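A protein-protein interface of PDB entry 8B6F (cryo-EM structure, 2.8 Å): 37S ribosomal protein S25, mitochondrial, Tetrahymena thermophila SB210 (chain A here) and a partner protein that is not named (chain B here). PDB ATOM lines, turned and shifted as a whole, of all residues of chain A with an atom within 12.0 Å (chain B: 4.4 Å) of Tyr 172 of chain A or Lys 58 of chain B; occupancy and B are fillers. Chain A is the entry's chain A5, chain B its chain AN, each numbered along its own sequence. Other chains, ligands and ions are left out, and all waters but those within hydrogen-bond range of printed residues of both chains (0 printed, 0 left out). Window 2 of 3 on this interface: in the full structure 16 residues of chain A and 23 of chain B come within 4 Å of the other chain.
The guanidinium group (NH2) of Arg 120 of chain B is in salt-bridge range of the side-chain carboxylate (OE1) of Glu 169 of chain A (3.2 Å).
The side-chain amino group of Lys 60 of chain B lies within salt-bridge range of the side-chain carboxylate of Glu 123 of chain B, 2.5 Å away. The side-chain amide nitrogen (ND2) of Asn 173 of chain A lies within hydrogen-bond range of the side-chain carboxylate (OE1) of Glu 169 of chain A.
Among the printed residues, merely in contact across the chains: Ile 168 of chain A with Glu 123 of chain B, Tyr 172 of chain A with Lys 58 of chain B, Tyr 172 of chain A with Lys 60 of chain B, Tyr 172 of chain A with Arg 120 of chain B and Tyr 172 of chain A with Glu 123 of chain B.
Of the printed residues of chain B, Ile 168 of chain A touches Glu 123 (3.2 Å). Printed residues of chain B within 4 Å of Glu 169 of chain A: Arg 120 (3.2 Å). Tyr 172 of chain A touches four residues of chain B. No residue of chain A comes within 4 Å of Thr 57 of chain B. Of the printed residues of chain A, Lys 58 of chain B touches Tyr 172. No residue of chain A comes within 4 Å of Leu 59 of chain B. No residue of chain A comes within 4 Å of Val 119 of chain B. Of the printed residues of chain A, Glu 123 of chain B touches Ile 168 and Tyr 172. The nearest residue of chain B that does not touch Tyr 172 of chain A is Val 119 of chain B (4.1 Å). The nearest printed residue of chain B that does not touch Glu 169 of chain A is Glu 123 of chain B (8.1 Å).
Of the 13 printed residues of chain A, 3 touch a printed residue of chain B. Among the printed residues, Asp or Glu carboxylates within 4 Å of a Lys or Arg side-chain nitrogen of the other chain: Glu 169 of chain A with Arg 120 of chain B.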
ATOM      1  N   TRP A 164      -1.719 -30.097 -32.156  1.00  0.00           N
ATOM      2  CA  TRP A 164      -2.473 -30.969 -31.265  1.00  0.00           C
ATOM      3  C   TRP A 164      -1.551 -31.818 -30.400  1.00  0.00           C
ATOM      4  O   TRP A 164      -1.908 -32.181 -29.275  1.00  0.00           O
ATOM      5  CB  TRP A 164      -3.409 -31.862 -32.086  1.00  0.00           C
ATOM      6  CG  TRP A 164      -4.060 -32.953 -31.299  1.00  0.00           C
ATOM      7  CD1 TRP A 164      -5.295 -32.925 -30.730  1.00  0.00           C
ATOM      8  CD2 TRP A 164      -3.507 -34.240 -31.000  1.00  0.00           C
ATOM      9  NE1 TRP A 164      -5.547 -34.115 -30.090  1.00  0.00           N
ATOM     10  CE2 TRP A 164      -4.464 -34.939 -30.242  1.00  0.00           C
ATOM     11  CE3 TRP A 164      -2.293 -34.868 -31.298  1.00  0.00           C
ATOM     12  CZ2 TRP A 164      -4.245 -36.234 -29.777  1.00  0.00           C
ATOM     13  CZ3 TRP A 164      -2.078 -36.152 -30.836  1.00  0.00           C
ATOM     14  CH2 TRP A 164      -3.050 -36.823 -30.084  1.00  0.00           C
ATOM     15  N   SER A 165      -0.360 -32.135 -30.911  1.00  0.00           N
ATOM     16  CA  SER A 165       0.513 -33.079 -30.217  1.00  0.00           C
ATOM     17  C   SER A 165       0.927 -32.558 -28.845  1.00  0.00           C
ATOM     18  O   SER A 165       0.936 -33.314 -27.868  1.00  0.00           O
ATOM     19  CB  SER A 165       1.747 -33.371 -31.070  1.00  0.00           C
ATOM     20  OG  SER A 165       1.393 -34.019 -32.279  1.00  0.00           O
ATOM     21  N   VAL A 166       1.277 -31.278 -28.752  1.00  0.00           N
ATOM     22  CA  VAL A 166       1.776 -30.693 -27.512  1.00  0.00           C
ATOM     23  C   VAL A 166       1.090 -29.355 -27.290  1.00  0.00           C
ATOM     24  O   VAL A 166       0.888 -28.584 -28.234  1.00  0.00           O
ATOM     25  CB  VAL A 166       3.310 -30.525 -27.536  1.00  0.00           C
ATOM     26  CG1 VAL A 166       3.983 -31.832 -27.926  1.00  0.00           C
ATOM     27  CG2 VAL A 166       3.718 -29.411 -28.480  1.00  0.00           C
ATOM     28  N   SER A 167       0.728 -29.081 -26.040  1.00  0.00           N
ATOM     29  CA  SER A 167       0.098 -27.810 -25.691  1.00  0.00           C
ATOM     30  C   SER A 167       0.285 -27.583 -24.198  1.00  0.00           C
ATOM     31  O   SER A 167      -0.297 -28.308 -23.387  1.00  0.00           O
ATOM     32  CB  SER A 167      -1.377 -27.817 -26.069  1.00  0.00           C
ATOM     33  OG  SER A 167      -2.002 -26.598 -25.711  1.00  0.00           O
ATOM     34  N   ILE A 168       1.090 -26.579 -23.842  1.00  0.00           N
ATOM     35  CA  ILE A 168       1.293 -26.249 -22.434  1.00  0.00           C
ATOM     36  C   ILE A 168      -0.006 -25.762 -21.810  1.00  0.00           C
ATOM     37  O   ILE A 168      -0.269 -26.010 -20.628  1.00  0.00           O
ATOM     38  CB  ILE A 168       2.423 -25.212 -22.283  1.00  0.00           C
ATOM     39  CG1 ILE A 168       2.846 -25.082 -20.817  1.00  0.00           C
ATOM     40  CG2 ILE A 168       1.996 -23.855 -22.825  1.00  0.00           C
ATOM     41  CD1 ILE A 168       3.530 -26.313 -20.257  1.00  0.00           C
ATOM     42  N   GLU A 169      -0.835 -25.060 -22.584  1.00  0.00           N
ATOM     43  CA  GLU A 169      -2.145 -24.654 -22.087  1.00  0.00           C
ATOM     44  C   GLU A 169      -2.988 -25.866 -21.722  1.00  0.00           C
ATOM     45  O   GLU A 169      -3.656 -25.877 -20.681  1.00  0.00           O
ATOM     46  CB  GLU A 169      -2.860 -23.803 -23.135  1.00  0.00           C
ATOM     47  CG  GLU A 169      -2.314 -22.392 -23.266  1.00  0.00           C
ATOM     48  CD  GLU A 169      -2.608 -21.541 -22.047  1.00  0.00           C
ATOM     49  OE1 GLU A 169      -3.295 -22.033 -21.128  1.00  0.00           O
ATOM     50  OE2 GLU A 169      -2.153 -20.378 -22.009  1.00  0.00           O
ATOM     51  N   GLU A 170      -2.970 -26.901 -22.563  1.00  0.00           N
ATOM     52  CA  GLU A 170      -3.680 -28.130 -22.227  1.00  0.00           C
ATOM     53  C   GLU A 170      -3.083 -28.781 -20.988  1.00  0.00           C
ATOM     54  O   GLU A 170      -3.815 -29.315 -20.146  1.00  0.00           O
ATOM     55  CB  GLU A 170      -3.640 -29.095 -23.413  1.00  0.00           C
ATOM     56  CG  GLU A 170      -4.266 -30.460 -23.141  1.00  0.00           C
ATOM     57  CD  GLU A 170      -5.730 -30.373 -22.754  1.00  0.00           C
ATOM     58  OE1 GLU A 170      -6.331 -29.292 -22.931  1.00  0.00           O
ATOM     59  OE2 GLU A 170      -6.283 -31.387 -22.276  1.00  0.00           O
ATOM     60  N   LYS A 171      -1.756 -28.756 -20.860  1.00  0.00           N
ATOM     61  CA  LYS A 171      -1.123 -29.357 -19.691  1.00  0.00           C
ATOM     62  C   LYS A 171      -1.578 -28.680 -18.404  1.00  0.00           C
ATOM     63  O   LYS A 171      -1.828 -29.352 -17.397  1.00  0.00           O
ATOM     64  CB  LYS A 171       0.399 -29.279 -19.824  1.00  0.00           C
ATOM     65  CG  LYS A 171       0.985 -30.215 -20.871  1.00  0.00           C
ATOM     66  CD  LYS A 171       0.909 -31.666 -20.427  1.00  0.00           C
ATOM     67  CE  LYS A 171       1.549 -32.588 -21.450  1.00  0.00           C
ATOM     68  NZ  LYS A 171       1.523 -34.009 -21.008  1.00  0.00           N
ATOM     69  N   TYR A 172      -1.684 -27.352 -18.413  1.00  0.00           N
ATOM     70  CA  TYR A 172      -1.992 -26.599 -17.205  1.00  0.00           C
ATOM     71  C   TYR A 172      -3.481 -26.346 -17.003  1.00  0.00           C
ATOM     72  O   TYR A 172      -3.869 -25.902 -15.919  1.00  0.00           O
ATOM     73  CB  TYR A 172      -1.247 -25.262 -17.216  1.00  0.00           C
ATOM     74  CG  TYR A 172       0.129 -25.354 -16.605  1.00  0.00           C
ATOM     75  CD1 TYR A 172       1.229 -25.714 -17.370  1.00  0.00           C
ATOM     76  CD2 TYR A 172       0.325 -25.095 -15.257  1.00  0.00           C
ATOM     77  CE1 TYR A 172       2.487 -25.807 -16.809  1.00  0.00           C
ATOM     78  CE2 TYR A 172       1.577 -25.187 -14.687  1.00  0.00           C
ATOM     79  CZ  TYR A 172       2.654 -25.543 -15.468  1.00  0.00           C
ATOM     80  OH  TYR A 172       3.905 -25.634 -14.903  1.00  0.00           O
ATOM     81  N   ASN A 173      -4.319 -26.610 -18.002  1.00  0.00           N
ATOM     82  CA  ASN A 173      -5.771 -26.479 -17.875  1.00  0.00           C
ATOM     83  C   ASN A 173      -6.431 -27.707 -18.486  1.00  0.00           C
ATOM     84  O   ASN A 173      -7.041 -27.633 -19.558  1.00  0.00           O
ATOM     85  CB  ASN A 173      -6.270 -25.199 -18.546  1.00  0.00           C
ATOM     86  CG  ASN A 173      -5.652 -23.951 -17.951  1.00  0.00           C
ATOM     87  OD1 ASN A 173      -5.345 -23.903 -16.761  1.00  0.00           O
ATOM     88  ND2 ASN A 173      -5.470 -22.928 -18.778  1.00  0.00           N
ATOM     89  N   PRO A 174      -6.324 -28.858 -17.826  1.00  0.00           N
ATOM     90  CA  PRO A 174      -6.878 -30.086 -18.408  1.00  0.00           C
ATOM     91  C   PRO A 174      -8.379 -29.976 -18.628  1.00  0.00           C
ATOM     92  O   PRO A 174      -9.103 -29.382 -17.827  1.00  0.00           O
ATOM     93  CB  PRO A 174      -6.538 -31.161 -17.368  1.00  0.00           C
ATOM     94  CG  PRO A 174      -5.444 -30.577 -16.542  1.00  0.00           C
ATOM     95  CD  PRO A 174      -5.686 -29.105 -16.523  1.00  0.00           C
ATOM     96  N   GLU A 175      -8.842 -30.562 -19.728  1.00  0.00           N
ATOM     97  CA  GLU A 175     -10.261 -30.663 -20.041  1.00  0.00           C
ATOM     98  C   GLU A 175     -10.617 -32.140 -20.109  1.00  0.00           C
ATOM     99  O   GLU A 175     -10.038 -32.881 -20.909  1.00  0.00           O
ATOM    100  CB  GLU A 175     -10.588 -29.960 -21.360  1.00  0.00           C
ATOM    101  CG  GLU A 175     -12.061 -29.998 -21.747  1.00  0.00           C
ATOM    102  CD  GLU A 175     -12.947 -29.232 -20.781  1.00  0.00           C
ATOM    103  OE1 GLU A 175     -12.408 -28.528 -19.900  1.00  0.00           O
ATOM    104  OE2 GLU A 175     -14.185 -29.334 -20.904  1.00  0.00           O
ATOM    105  N   LEU A 176     -11.563 -32.564 -19.277  1.00  0.00           N
ATOM    106  CA  LEU A 176     -11.887 -33.972 -19.124  1.00  0.00           C
ATOM    107  C   LEU A 176     -13.305 -34.249 -19.595  1.00  0.00           C
ATOM    108  O   LEU A 176     -14.183 -33.384 -19.525  1.00  0.00           O
ATOM    109  CB  LEU A 176     -11.750 -34.420 -17.664  1.00  0.00           C
ATOM    110  CG  LEU A 176     -10.401 -34.181 -16.988  1.00  0.00           C
ATOM    111  CD1 LEU A 176     -10.433 -34.735 -15.578  1.00  0.00           C
ATOM    112  CD2 LEU A 176      -9.262 -34.793 -17.781  1.00  0.00           C
ATOM    113  N   THR B  57       5.010 -22.958  -5.960  1.00  0.00           N
ATOM    114  CA  THR B  57       3.579 -22.921  -6.206  1.00  0.00           C
ATOM    115  C   THR B  57       3.322 -22.908  -7.710  1.00  0.00           C
ATOM    116  O   THR B  57       4.244 -22.945  -8.528  1.00  0.00           O
ATOM    117  CB  THR B  57       2.945 -21.706  -5.525  1.00  0.00           C
ATOM    118  OG1 THR B  57       3.564 -20.505  -6.004  1.00  0.00           O
ATOM    119  CG2 THR B  57       3.111 -21.793  -4.017  1.00  0.00           C
ATOM    120  N   LYS B  58       2.044 -22.854  -8.078  1.00  0.00           N
ATOM    121  CA  LYS B  58       1.635 -22.836  -9.480  1.00  0.00           C
ATOM    122  C   LYS B  58       2.077 -24.099 -10.213  1.00  0.00           C
ATOM    123  O   LYS B  58       2.312 -24.075 -11.423  1.00  0.00           O
ATOM    124  CB  LYS B  58       2.180 -21.595 -10.196  1.00  0.00           C
ATOM    125  CG  LYS B  58       1.860 -20.282  -9.498  1.00  0.00           C
ATOM    126  CD  LYS B  58       2.475 -19.100 -10.235  1.00  0.00           C
ATOM    127  CE  LYS B  58       2.195 -17.794  -9.506  1.00  0.00           C
ATOM    128  NZ  LYS B  58       2.792 -16.621 -10.206  1.00  0.00           N
ATOM    129  N   LEU B  59       2.201 -25.208  -9.490  1.00  0.00           N
ATOM    130  CA  LEU B  59       2.555 -26.473 -10.110  1.00  0.00           C
ATOM    131  C   LEU B  59       1.340 -27.091 -10.793  1.00  0.00           C
ATOM    132  O   LEU B  59       0.190 -26.779 -10.479  1.00  0.00           O
ATOM    133  CB  LEU B  59       3.113 -27.448  -9.070  1.00  0.00           C
ATOM    134  CG  LEU B  59       4.477 -27.116  -8.461  1.00  0.00           C
ATOM    135  CD1 LEU B  59       4.825 -28.124  -7.381  1.00  0.00           C
ATOM    136  CD2 LEU B  59       5.566 -27.080  -9.524  1.00  0.00           C
ATOM    137  N   LYS B  60       1.613 -27.981 -11.742  1.00  0.00           N
ATOM    138  CA  LYS B  60       0.544 -28.687 -12.431  1.00  0.00           C
ATOM    139  C   LYS B  60      -0.183 -29.616 -11.467  1.00  0.00           C
ATOM    140  O   LYS B  60       0.424 -30.202 -10.566  1.00  0.00           O
ATOM    141  CB  LYS B  60       1.098 -29.490 -13.605  1.00  0.00           C
ATOM    142  CG  LYS B  60       1.683 -28.641 -14.721  1.00  0.00           C
ATOM    143  CD  LYS B  60       2.020 -29.479 -15.946  1.00  0.00           C
ATOM    144  CE  LYS B  60       3.063 -30.544 -15.645  1.00  0.00           C
ATOM    145  NZ  LYS B  60       4.313 -29.971 -15.080  1.00  0.00           N
ATOM    146  N   VAL B 119       8.634 -22.484 -13.452  1.00  0.00           N
ATOM    147  CA  VAL B 119       8.539 -23.847 -13.967  1.00  0.00           C
ATOM    148  C   VAL B 119       7.838 -23.865 -15.319  1.00  0.00           C
ATOM    149  O   VAL B 119       8.243 -24.596 -16.231  1.00  0.00           O
ATOM    150  CB  VAL B 119       7.826 -24.751 -12.946  1.00  0.00           C
ATOM    151  CG1 VAL B 119       7.695 -26.170 -13.482  1.00  0.00           C
ATOM    152  CG2 VAL B 119       8.574 -24.749 -11.624  1.00  0.00           C
ATOM    153  N   ARG B 120       6.783 -23.065 -15.476  1.00  0.00           N
ATOM    154  CA  ARG B 120       6.066 -23.042 -16.746  1.00  0.00           C
ATOM    155  C   ARG B 120       6.951 -22.516 -17.867  1.00  0.00           C
ATOM    156  O   ARG B 120       6.944 -23.059 -18.977  1.00  0.00           O
ATOM    157  CB  ARG B 120       4.798 -22.199 -16.618  1.00  0.00           C
ATOM    158  CG  ARG B 120       3.849 -22.339 -17.798  1.00  0.00           C
ATOM    159  CD  ARG B 120       2.464 -21.817 -17.459  1.00  0.00           C
ATOM    160  NE  ARG B 120       1.536 -21.976 -18.571  1.00  0.00           N
ATOM    161  CZ  ARG B 120       0.234 -21.738 -18.500  1.00  0.00           C
ATOM    162  NH1 ARG B 120      -0.335 -21.335 -17.376  1.00  0.00           N
ATOM    163  NH2 ARG B 120      -0.517 -21.908 -19.583  1.00  0.00           N
ATOM    164  N   GLU B 123       9.389 -25.245 -18.770  1.00  0.00           N
ATOM    165  CA  GLU B 123       8.743 -26.263 -19.593  1.00  0.00           C
ATOM    166  C   GLU B 123       8.558 -25.777 -21.023  1.00  0.00           C
ATOM    167  O   GLU B 123       8.768 -26.536 -21.977  1.00  0.00           O
ATOM    168  CB  GLU B 123       7.398 -26.657 -18.986  1.00  0.00           C
ATOM    169  CG  GLU B 123       7.519 -27.450 -17.701  1.00  0.00           C
ATOM    170  CD  GLU B 123       6.171 -27.806 -17.114  1.00  0.00           C
ATOM    171  OE1 GLU B 123       5.144 -27.390 -17.689  1.00  0.00           O
ATOM    172  OE2 GLU B 123       6.135 -28.504 -16.080  1.00  0.00           O
